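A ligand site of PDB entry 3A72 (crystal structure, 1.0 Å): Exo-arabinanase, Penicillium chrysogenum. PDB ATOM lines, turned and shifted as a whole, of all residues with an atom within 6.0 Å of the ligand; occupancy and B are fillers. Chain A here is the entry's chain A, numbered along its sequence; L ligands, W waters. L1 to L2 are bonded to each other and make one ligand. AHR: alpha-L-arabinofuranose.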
ATOM      1  N   LEU A  24       3.655  16.163   8.883  1.00  0.00           N
ATOM      2  CA  LEU A  24       3.182  14.795   8.952  1.00  0.00           C
ATOM      3  C   LEU A  24       1.679  14.794   9.156  1.00  0.00           C
ATOM      4  O   LEU A  24       1.148  15.794   9.678  1.00  0.00           O
ATOM      5  CB  LEU A  24       3.811  14.059  10.179  1.00  0.00           C
ATOM      6  CG  LEU A  24       3.837  12.528  10.092  1.00  0.00           C
ATOM      7  CD1 LEU A  24       4.870  12.034   9.090  1.00  0.00           C
ATOM      8  CD2 LEU A  24       4.109  11.934  11.480  1.00  0.00           C
ATOM      9  N   TYR A  25       0.984  13.721   8.814  1.00  0.00           N
ATOM     10  CA  TYR A  25      -0.377  13.462   9.256  1.00  0.00           C
ATOM     11  C   TYR A  25      -1.364  14.420   8.579  1.00  0.00           C
ATOM     12  O   TYR A  25      -1.929  15.331   9.209  1.00  0.00           O
ATOM     13  CB  TYR A  25      -0.482  13.504  10.777  1.00  0.00           C
ATOM     14  CG  TYR A  25      -1.632  12.683  11.346  1.00  0.00           C
ATOM     15  CD1 TYR A  25      -1.370  11.461  11.976  1.00  0.00           C
ATOM     16  CD2 TYR A  25      -2.965  13.093  11.219  1.00  0.00           C
ATOM     17  CE1 TYR A  25      -2.405  10.677  12.502  1.00  0.00           C
ATOM     18  CE2 TYR A  25      -4.003  12.305  11.754  1.00  0.00           C
ATOM     19  CZ  TYR A  25      -3.709  11.131  12.370  1.00  0.00           C
ATOM     20  OH  TYR A  25      -4.695  10.330  12.935  1.00  0.00           O
ATOM     21  N   GLU A  41       0.225  18.026  11.148  1.00  0.00           N
ATOM     22  CA  GLU A  41       1.177  18.235  12.217  1.00  0.00           C
ATOM     23  C   GLU A  41       2.325  19.092  11.687  1.00  0.00           C
ATOM     24  O   GLU A  41       2.966  18.728  10.684  1.00  0.00           O
ATOM     25  CB  GLU A  41       1.762  16.916  12.709  1.00  0.00           C
ATOM     26  CG  GLU A  41       0.728  15.952  13.311  1.00  0.00           C
ATOM     27  CD  GLU A  41       1.229  14.573  13.616  1.00  0.00           C
ATOM     28  OE1 GLU A  41       2.427  14.274  13.316  1.00  0.00           O
ATOM     29  OE2 GLU A  41       0.419  13.734  14.110  1.00  0.00           O
ATOM     30  N   TYR A  43       5.726  20.924  12.557  1.00  0.00           N
ATOM     31  CA  TYR A  43       6.845  20.769  13.526  1.00  0.00           C
ATOM     32  C   TYR A  43       7.742  22.011  13.514  1.00  0.00           C
ATOM     33  O   TYR A  43       8.924  21.978  13.230  1.00  0.00           O
ATOM     34  CB  TYR A  43       7.620  19.502  13.243  1.00  0.00           C
ATOM     35  CG  TYR A  43       6.862  18.221  13.479  1.00  0.00           C
ATOM     36  CD1 TYR A  43       7.115  17.452  14.588  1.00  0.00           C
ATOM     37  CD2 TYR A  43       5.874  17.771  12.573  1.00  0.00           C
ATOM     38  CE1 TYR A  43       6.436  16.265  14.844  1.00  0.00           C
ATOM     39  CE2 TYR A  43       5.193  16.580  12.838  1.00  0.00           C
ATOM     40  CZ  TYR A  43       5.471  15.856  13.974  1.00  0.00           C
ATOM     41  OH  TYR A  43       4.828  14.672  14.252  1.00  0.00           O
ATOM     42  N   TYR A  81      -0.017  16.685  17.620  1.00  0.00           N
ATOM     43  CA  TYR A  81      -0.231  15.441  16.898  1.00  0.00           C
ATOM     44  C   TYR A  81      -1.709  15.281  16.446  1.00  0.00           C
ATOM     45  O   TYR A  81      -2.643  15.647  17.178  1.00  0.00           O
ATOM     46  CB  TYR A  81       0.104  14.214  17.704  1.00  0.00           C
ATOM     47  CG  TYR A  81       1.573  13.897  17.934  1.00  0.00           C
ATOM     48  CD1 TYR A  81       2.618  14.559  17.263  1.00  0.00           C
ATOM     49  CD2 TYR A  81       1.912  12.866  18.832  1.00  0.00           C
ATOM     50  CE1 TYR A  81       3.948  14.210  17.508  1.00  0.00           C
ATOM     51  CE2 TYR A  81       3.202  12.529  19.072  1.00  0.00           C
ATOM     52  CZ  TYR A  81       4.234  13.220  18.400  1.00  0.00           C
ATOM     53  OH  TYR A  81       5.571  12.875  18.603  1.00  0.00           O
ATOM     54  N   GLN A  82      -1.856  14.670  15.285  1.00  0.00           N
ATOM     55  CA  GLN A  82      -3.084  13.976  14.905  1.00  0.00           C
ATOM     56  C   GLN A  82      -4.327  14.880  14.871  1.00  0.00           C
ATOM     57  O   GLN A  82      -5.332  14.606  15.470  1.00  0.00           O
ATOM     58  CB  GLN A  82      -3.292  12.782  15.840  1.00  0.00           C
ATOM     59  CG  GLN A  82      -2.144  11.793  15.707  1.00  0.00           C
ATOM     60  CD  GLN A  82      -1.644  11.198  17.008  1.00  0.00           C
ATOM     61  OE1 GLN A  82      -2.374  11.138  18.019  1.00  0.00           O
ATOM     62  NE2 GLN A  82      -0.424  10.699  16.984  1.00  0.00           N
ATOM     63  N   ALA A 140       3.392  10.442  25.067  1.00  0.00           N
ATOM     64  CA  ALA A 140       3.124  10.383  23.629  1.00  0.00           C
ATOM     65  C   ALA A 140       4.174   9.611  22.867  1.00  0.00           C
ATOM     66  O   ALA A 140       4.759  10.113  21.907  1.00  0.00           O
ATOM     67  CB  ALA A 140       2.993  11.788  23.119  1.00  0.00           C
ATOM     68  N   ARG A 141       4.377   8.353  23.283  1.00  0.00           N
ATOM     69  CA  ARG A 141       5.217   7.428  22.506  1.00  0.00           C
ATOM     70  C   ARG A 141       4.471   6.078  22.419  1.00  0.00           C
ATOM     71  O   ARG A 141       3.869   5.646  23.394  1.00  0.00           O
ATOM     72  CB  ARG A 141       6.591   7.181  23.127  1.00  0.00           C
ATOM     73  CG  ARG A 141       7.461   8.415  23.127  1.00  0.00           C
ATOM     74  CD  ARG A 141       8.867   8.078  23.625  1.00  0.00           C
ATOM     75  NE  ARG A 141       9.769   9.247  23.626  1.00  0.00           N
ATOM     76  CZ  ARG A 141       9.938  10.111  24.592  1.00  0.00           C
ATOM     77  NH1 ARG A 141       9.288   9.978  25.737  1.00  0.00           N
ATOM     78  NH2 ARG A 141      10.777  11.130  24.427  1.00  0.00           N
ATOM     79  N   PRO A 142       4.548   5.424  21.265  1.00  0.00           N
ATOM     80  CA  PRO A 142       3.789   4.184  21.021  1.00  0.00           C
ATOM     81  C   PRO A 142       4.521   2.962  21.541  1.00  0.00           C
ATOM     82  O   PRO A 142       4.827   2.058  20.787  1.00  0.00           O
ATOM     83  CB  PRO A 142       3.586   4.169  19.530  1.00  0.00           C
ATOM     84  CG  PRO A 142       4.894   4.764  19.036  1.00  0.00           C
ATOM     85  CD  PRO A 142       5.131   5.946  20.020  1.00  0.00           C
ATOM     86  N   TRP A 150      -4.608   8.689  21.127  1.00  0.00           N
ATOM     87  CA  TRP A 150      -4.130   9.114  19.819  1.00  0.00           C
ATOM     88  C   TRP A 150      -5.242   9.188  18.769  1.00  0.00           C
ATOM     89  O   TRP A 150      -6.219   8.419  18.819  1.00  0.00           O
ATOM     90  CB  TRP A 150      -3.177   8.111  19.309  1.00  0.00           C
ATOM     91  CG  TRP A 150      -2.102   7.417  20.063  1.00  0.00           C
ATOM     92  CD1 TRP A 150      -2.151   6.160  20.593  1.00  0.00           C
ATOM     93  CD2 TRP A 150      -0.771   7.901  20.296  1.00  0.00           C
ATOM     94  NE1 TRP A 150      -0.951   5.898  21.138  1.00  0.00           N
ATOM     95  CE2 TRP A 150      -0.062   6.904  20.958  1.00  0.00           C
ATOM     96  CE3 TRP A 150      -0.122   9.100  20.015  1.00  0.00           C
ATOM     97  CZ2 TRP A 150       1.264   7.012  21.299  1.00  0.00           C
ATOM     98  CZ3 TRP A 150       1.227   9.221  20.323  1.00  0.00           C
ATOM     99  CH2 TRP A 150       1.886   8.175  20.961  1.00  0.00           C
ATOM    100  N   GLU A 151      -5.032   9.986  17.731  1.00  0.00           N
ATOM    101  CA  GLU A 151      -5.638   9.729  16.406  1.00  0.00           C
ATOM    102  C   GLU A 151      -7.178   9.855  16.386  1.00  0.00           C
ATOM    103  O   GLU A 151      -7.871   8.917  15.959  1.00  0.00           O
ATOM    104  CB  GLU A 151      -5.178   8.399  15.861  1.00  0.00           C
ATOM    105  CG  GLU A 151      -3.670   8.327  15.623  1.00  0.00           C
ATOM    106  CD  GLU A 151      -3.045   6.999  15.896  1.00  0.00           C
ATOM    107  OE1 GLU A 151      -3.662   6.032  16.326  1.00  0.00           O
ATOM    108  OE2 GLU A 151      -1.756   6.879  15.679  1.00  0.00           O
ATOM    109  N   SER A 166      -7.524   5.890  19.228  1.00  0.00           N
ATOM    110  CA  SER A 166      -6.698   4.818  19.729  1.00  0.00           C
ATOM    111  C   SER A 166      -6.344   5.069  21.199  1.00  0.00           C
ATOM    112  O   SER A 166      -6.082   6.226  21.565  1.00  0.00           O
ATOM    113  CB  SER A 166      -5.423   4.678  18.921  1.00  0.00           C
ATOM    114  OG  SER A 166      -5.695   4.602  17.531  1.00  0.00           O
ATOM    115  N   GLN A 168      -4.244   3.641  24.762  1.00  0.00           N
ATOM    116  CA  GLN A 168      -3.344   2.805  25.494  1.00  0.00           C
ATOM    117  C   GLN A 168      -3.619   2.803  27.006  1.00  0.00           C
ATOM    118  O   GLN A 168      -2.851   2.181  27.766  1.00  0.00           O
ATOM    119  CB  GLN A 168      -1.887   3.190  25.250  1.00  0.00           C
ATOM    120  CG  GLN A 168      -1.425   2.889  23.807  1.00  0.00           C
ATOM    121  CD  GLN A 168       0.049   3.037  23.617  1.00  0.00           C
ATOM    122  OE1 GLN A 168       0.898   2.577  24.497  1.00  0.00           O
ATOM    123  NE2 GLN A 168       0.477   3.519  22.550  1.00  0.00           N
ATOM    124  N   GLN A 176      -2.595  -1.789  23.001  1.00  0.00           N
ATOM    125  CA  GLN A 176      -3.414  -0.685  22.528  1.00  0.00           C
ATOM    126  C   GLN A 176      -4.782  -1.242  22.173  1.00  0.00           C
ATOM    127  O   GLN A 176      -4.889  -2.389  21.729  1.00  0.00           O
ATOM    128  CB  GLN A 176      -2.779   0.065  21.368  1.00  0.00           C
ATOM    129  CG  GLN A 176      -3.492   1.348  20.972  1.00  0.00           C
ATOM    130  CD  GLN A 176      -2.730   2.114  19.910  1.00  0.00           C
ATOM    131  OE1 GLN A 176      -2.897   1.768  18.673  1.00  0.00           O
ATOM    132  NE2 GLN A 176      -1.977   3.048  20.272  1.00  0.00           N
ATOM    133  N   ARG A 204      -1.686  -4.475  18.767  1.00  0.00           N
ATOM    134  CA  ARG A 204      -1.875  -3.016  18.787  1.00  0.00           C
ATOM    135  C   ARG A 204      -2.705  -2.638  17.557  1.00  0.00           C
ATOM    136  O   ARG A 204      -2.214  -2.066  16.570  1.00  0.00           O
ATOM    137  CB  ARG A 204      -0.518  -2.246  18.806  1.00  0.00           C
ATOM    138  CG  ARG A 204       0.258  -2.513  20.084  1.00  0.00           C
ATOM    139  CD  ARG A 204       1.690  -1.871  20.031  1.00  0.00           C
ATOM    140  NE  ARG A 204       1.599  -0.453  19.821  1.00  0.00           N
ATOM    141  CZ  ARG A 204       1.347   0.451  20.736  1.00  0.00           C
ATOM    142  NH1 ARG A 204       1.334   0.145  22.021  1.00  0.00           N
ATOM    143  NH2 ARG A 204       1.144   1.677  20.351  1.00  0.00           N
ATOM    144  N   PRO A 205      -4.024  -2.902  17.599  1.00  0.00           N
ATOM    145  CA  PRO A 205      -4.916  -2.291  16.607  1.00  0.00           C
ATOM    146  C   PRO A 205      -4.855  -0.781  16.786  1.00  0.00           C
ATOM    147  O   PRO A 205      -4.773  -0.283  17.945  1.00  0.00           O
ATOM    148  CB  PRO A 205      -6.261  -2.893  16.963  1.00  0.00           C
ATOM    149  CG  PRO A 205      -6.204  -3.081  18.456  1.00  0.00           C
ATOM    150  CD  PRO A 205      -4.795  -3.594  18.681  1.00  0.00           C
ATOM    151  N   GLY A 206      -4.928  -0.017  15.712  1.00  0.00           N
ATOM    152  CA  GLY A 206      -4.850   1.436  15.791  1.00  0.00           C
ATOM    153  C   GLY A 206      -5.389   2.097  14.555  1.00  0.00           C
ATOM    154  O   GLY A 206      -5.573   1.523  13.480  1.00  0.00           O
ATOM    155  N   MET A 207      -5.573   3.421  14.673  1.00  0.00           N
ATOM    156  CA  MET A 207      -5.778   4.358  13.597  1.00  0.00           C
ATOM    157  C   MET A 207      -7.122   4.168  12.907  1.00  0.00           C
ATOM    158  O   MET A 207      -7.220   3.874  11.725  1.00  0.00           O
ATOM    159  CB  MET A 207      -4.638   4.292  12.572  1.00  0.00           C
ATOM    160  CG  MET A 207      -3.266   4.420  13.241  1.00  0.00           C
ATOM    161  SD  MET A 207      -1.880   4.769  12.122  1.00  0.00           S
ATOM    162  CE  MET A 207      -2.127   6.535  11.882  1.00  0.00           C
ATOM    163  N   GLU A 223      -5.432  -0.263  11.154  1.00  0.00           N
ATOM    164  CA  GLU A 223      -4.253  -1.129  11.085  1.00  0.00           C
ATOM    165  C   GLU A 223      -4.329  -2.096  12.241  1.00  0.00           C
ATOM    166  O   GLU A 223      -4.636  -1.706  13.381  1.00  0.00           O
ATOM    167  CB  GLU A 223      -2.931  -0.339  11.082  1.00  0.00           C
ATOM    168  CG  GLU A 223      -2.679   0.448  12.375  1.00  0.00           C
ATOM    169  CD  GLU A 223      -1.367   1.197  12.407  1.00  0.00           C
ATOM    170  OE1 GLU A 223      -0.762   1.478  11.328  1.00  0.00           O
ATOM    171  OE2 GLU A 223      -0.952   1.517  13.562  1.00  0.00           O
ATOM    172  N   PHE A 235       1.395  -4.690  10.329  1.00  0.00           N
ATOM    173  CA  PHE A 235       0.239  -3.812  10.488  1.00  0.00           C
ATOM    174  C   PHE A 235      -0.721  -3.948   9.315  1.00  0.00           C
ATOM    175  O   PHE A 235      -1.092  -2.929   8.686  1.00  0.00           O
ATOM    176  CB  PHE A 235       0.688  -2.354  10.647  1.00  0.00           C
ATOM    177  CG  PHE A 235       1.460  -2.045  11.906  1.00  0.00           C
ATOM    178  CD1 PHE A 235       0.792  -1.673  13.030  1.00  0.00           C
ATOM    179  CD2 PHE A 235       2.833  -2.043  11.916  1.00  0.00           C
ATOM    180  CE1 PHE A 235       1.476  -1.290  14.220  1.00  0.00           C
ATOM    181  CE2 PHE A 235       3.523  -1.705  13.064  1.00  0.00           C
ATOM    182  CZ  PHE A 235       2.834  -1.284  14.183  1.00  0.00           C
ATOM    183  N   TYR A 314       2.498   8.606   5.246  1.00  0.00           N
ATOM    184  CA  TYR A 314       1.892   8.170   6.479  1.00  0.00           C
ATOM    185  C   TYR A 314       0.487   8.756   6.641  1.00  0.00           C
ATOM    186  O   TYR A 314       0.274   9.970   6.485  1.00  0.00           O
ATOM    187  CB  TYR A 314       2.739   8.654   7.635  1.00  0.00           C
ATOM    188  CG  TYR A 314       2.290   8.212   9.022  1.00  0.00           C
ATOM    189  CD1 TYR A 314       2.210   6.878   9.372  1.00  0.00           C
ATOM    190  CD2 TYR A 314       1.972   9.153   9.959  1.00  0.00           C
ATOM    191  CE1 TYR A 314       1.804   6.460  10.600  1.00  0.00           C
ATOM    192  CE2 TYR A 314       1.623   8.776  11.256  1.00  0.00           C
ATOM    193  CZ  TYR A 314       1.552   7.434  11.570  1.00  0.00           C
ATOM    194  OH  TYR A 314       1.244   7.048  12.863  1.00  0.00           O
ATOM    195  N   LEU A 337       6.995   9.071   8.108  1.00  0.00           N
ATOM    196  CA  LEU A 337       7.562   9.116   9.450  1.00  0.00           C
ATOM    197  C   LEU A 337       9.051   9.411   9.378  1.00  0.00           C
ATOM    198  O   LEU A 337       9.789   8.801   8.594  1.00  0.00           O
ATOM    199  CB  LEU A 337       7.360   7.741  10.134  1.00  0.00           C
ATOM    200  CG  LEU A 337       5.887   7.491  10.595  1.00  0.00           C
ATOM    201  CD1 LEU A 337       5.701   6.006  10.937  1.00  0.00           C
ATOM    202  CD2 LEU A 337       5.473   8.348  11.785  1.00  0.00           C
HETATM  203  O5  AHR L   1       2.716   7.074  16.846  1.00  0.00           O
HETATM  204  C5  AHR L   1       1.417   6.684  17.414  1.00  0.00           C
HETATM  205  C4  AHR L   1       1.107   5.290  16.959  1.00  0.00           C
HETATM  206  O4  AHR L   1       0.840   5.321  15.552  1.00  0.00           O
HETATM  207  C3  AHR L   1      -0.158   4.728  17.605  1.00  0.00           C
HETATM  208  O3  AHR L   1       0.180   4.064  18.831  1.00  0.00           O
HETATM  209  C2  AHR L   1      -0.664   3.744  16.527  1.00  0.00           C
HETATM  210  O2  AHR L   1      -2.084   3.624  16.483  1.00  0.00           O
HETATM  211  C1  AHR L   1      -0.078   4.274  15.217  1.00  0.00           C
HETATM  212  O1  AHR L   1       0.745   3.251  14.572  1.00  0.00           O
HETATM  213  O5  AHR L   2       1.229  11.233  14.629  1.00  0.00           O
HETATM  214  C5  AHR L   2       2.583  11.342  15.159  1.00  0.00           C
HETATM  215  C4  AHR L   2       3.117   9.950  15.410  1.00  0.00           C
HETATM  216  O4  AHR L   2       2.308   9.347  16.479  1.00  0.00           O
HETATM  217  C3  AHR L   2       4.498   9.972  16.045  1.00  0.00           C
HETATM  218  O3  AHR L   2       5.535  10.066  15.043  1.00  0.00           O
HETATM  219  C2  AHR L   2       4.540   8.579  16.696  1.00  0.00           C
HETATM  220  O2  AHR L   2       5.454   8.520  17.812  1.00  0.00           O
HETATM  221  C1  AHR L   2       3.098   8.390  17.182  1.00  0.00           C
HETATM  222  O   HOH W   1       6.535  12.520  14.438  1.00  0.00           O
HETATM  223  O   HOH W   2       3.261   2.359  15.886  1.00  0.00           O
HETATM  224  O   HOH W   3      -1.094   0.432  16.120  1.00  0.00           O
HETATM  225  O   HOH W   4       2.586   4.687  13.181  1.00  0.00           O
HETATM  226  O   HOH W   5       8.094   9.096  14.484  1.00  0.00           O
HETATM  227  O   HOH W   6       4.175   5.124  15.367  1.00  0.00           O
HETATM  228  O   HOH W   7       7.578   7.026  17.393  1.00  0.00           O
HETATM  229  O   HOH W   8       6.104  10.426  19.604  1.00  0.00           O
HETATM  230  O   HOH W   9      -0.337   8.628  14.387  1.00  0.00           O
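NH2 of Arg 204 sits at hydrogen-bond distance from O3 of AHR L1 (3.0 Å).
OE2 of Glu 223 sits at hydrogen-bond distance from O1 of AHR L1 (2.6 Å).
The side-chain hydroxyl (OH) of Tyr 314 lies within hydrogen-bond range of an oxygen (O4) of AHR L1 (3.2 Å).
The side-chain amide nitrogen of Gln 82 sits at hydrogen-bond distance from an oxygen (O5) of AHR L2.
An oxygen (O3) of AHR L1 sits at hydrogen-bond distance from the side-chain amide nitrogen (NE2) of Gln 176 (2.8 Å).
OE1 of Glu 151 is in hydrogen-bond range of O2 of AHR L1 (2.9 Å).
An oxygen (O5) of AHR L2 lies within hydrogen-bond range of the side-chain carboxylate of Glu 41 (2.7 Å).
The indole nitrogen of Trp 150 is in hydrogen-bond range of an oxygen (O3) of AHR L1, at 3.2 Å.
N of Glu 41 sits at hydrogen-bond distance from O of Leu 24 (2.8 Å).
OE1 of Glu 41 is in hydrogen-bond range of OH of Tyr 43 (2.6 Å).
The backbone NH (N) of Glu 151 lies within hydrogen-bond range of the side-chain amide oxygen (OE1) of Gln 82.
The backbone NH (N) of Gln 82 is in hydrogen-bond range of the side-chain carboxylate (OE2) of Glu 41.
O of Trp 150 lies within hydrogen-bond range of N of Ser 166 (2.9 Å).
NE2 of Gln 176 sits close to NE1 of Trp 150.
The indole nitrogen of Trp 150 sits close to the side-chain amide nitrogen of Gln 168 (3.1 Å).
The side-chain amide nitrogen (NE2) of Gln 176 lies close to the guanidinium group (NH2) of Arg 204 (3.4 Å).
Tyr 25 touches the ligand.
CD1 of Tyr 81 touches C5 of AHR L2, 3.8 Å away.
CD of Pro 142 touches O2 of AHR L2, at 3.4 Å.
Ser 166 touches the ligand.
NE2 of Gln 168 touches O3 of AHR L1, at 3.8 Å.
CA of Gly 206 touches O2 of AHR L1, 3.6 Å away.
CG of Met 207 touches O2 of AHR L1 (3.5 Å).
CD2 of Leu 337 touches O3 of AHR L2, 3.7 Å away.
Hydrophobic or aromatic side chains within 4 Å of the ligand: Tyr 25, Tyr 81, Pro 142, Trp 150, Met 207 and Leu 337.
Within 4 Å of the ligand: Tyr 25, Glu 41, Tyr 81, Gln 82, Pro 142, Trp 150, Glu 151, Ser 166, Gln 168, Gln 176, Arg 204, Gly 206, Met 207, Glu 223, Tyr 314 and Leu 337.
Water W8 lies within hydrogen-bond range of O of Ala 140, O2 of AHR L2 and OH of Tyr 81.
Water W4 lies within hydrogen-bond range of an oxygen (O1) of AHR L1 (2.7 Å) and the side-chain hydroxyl of Tyr 314 (2.7 Å).
Water W1 lies within hydrogen-bond range of an oxygen (O3) of AHR L2 (2.7 Å) and the side-chain hydroxyl (OH) of Tyr 43 (2.8 Å).
Water W9 lies within hydrogen-bond range of the side-chain carboxylate (OE2) of Glu 151 (2.6 Å), the side-chain hydroxyl (OH) of Tyr 314 (2.7 Å), an oxygen (O5) of AHR L2 (3.0 Å) and the side-chain amide nitrogen (NE2) of Gln 82 (3.3 Å).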
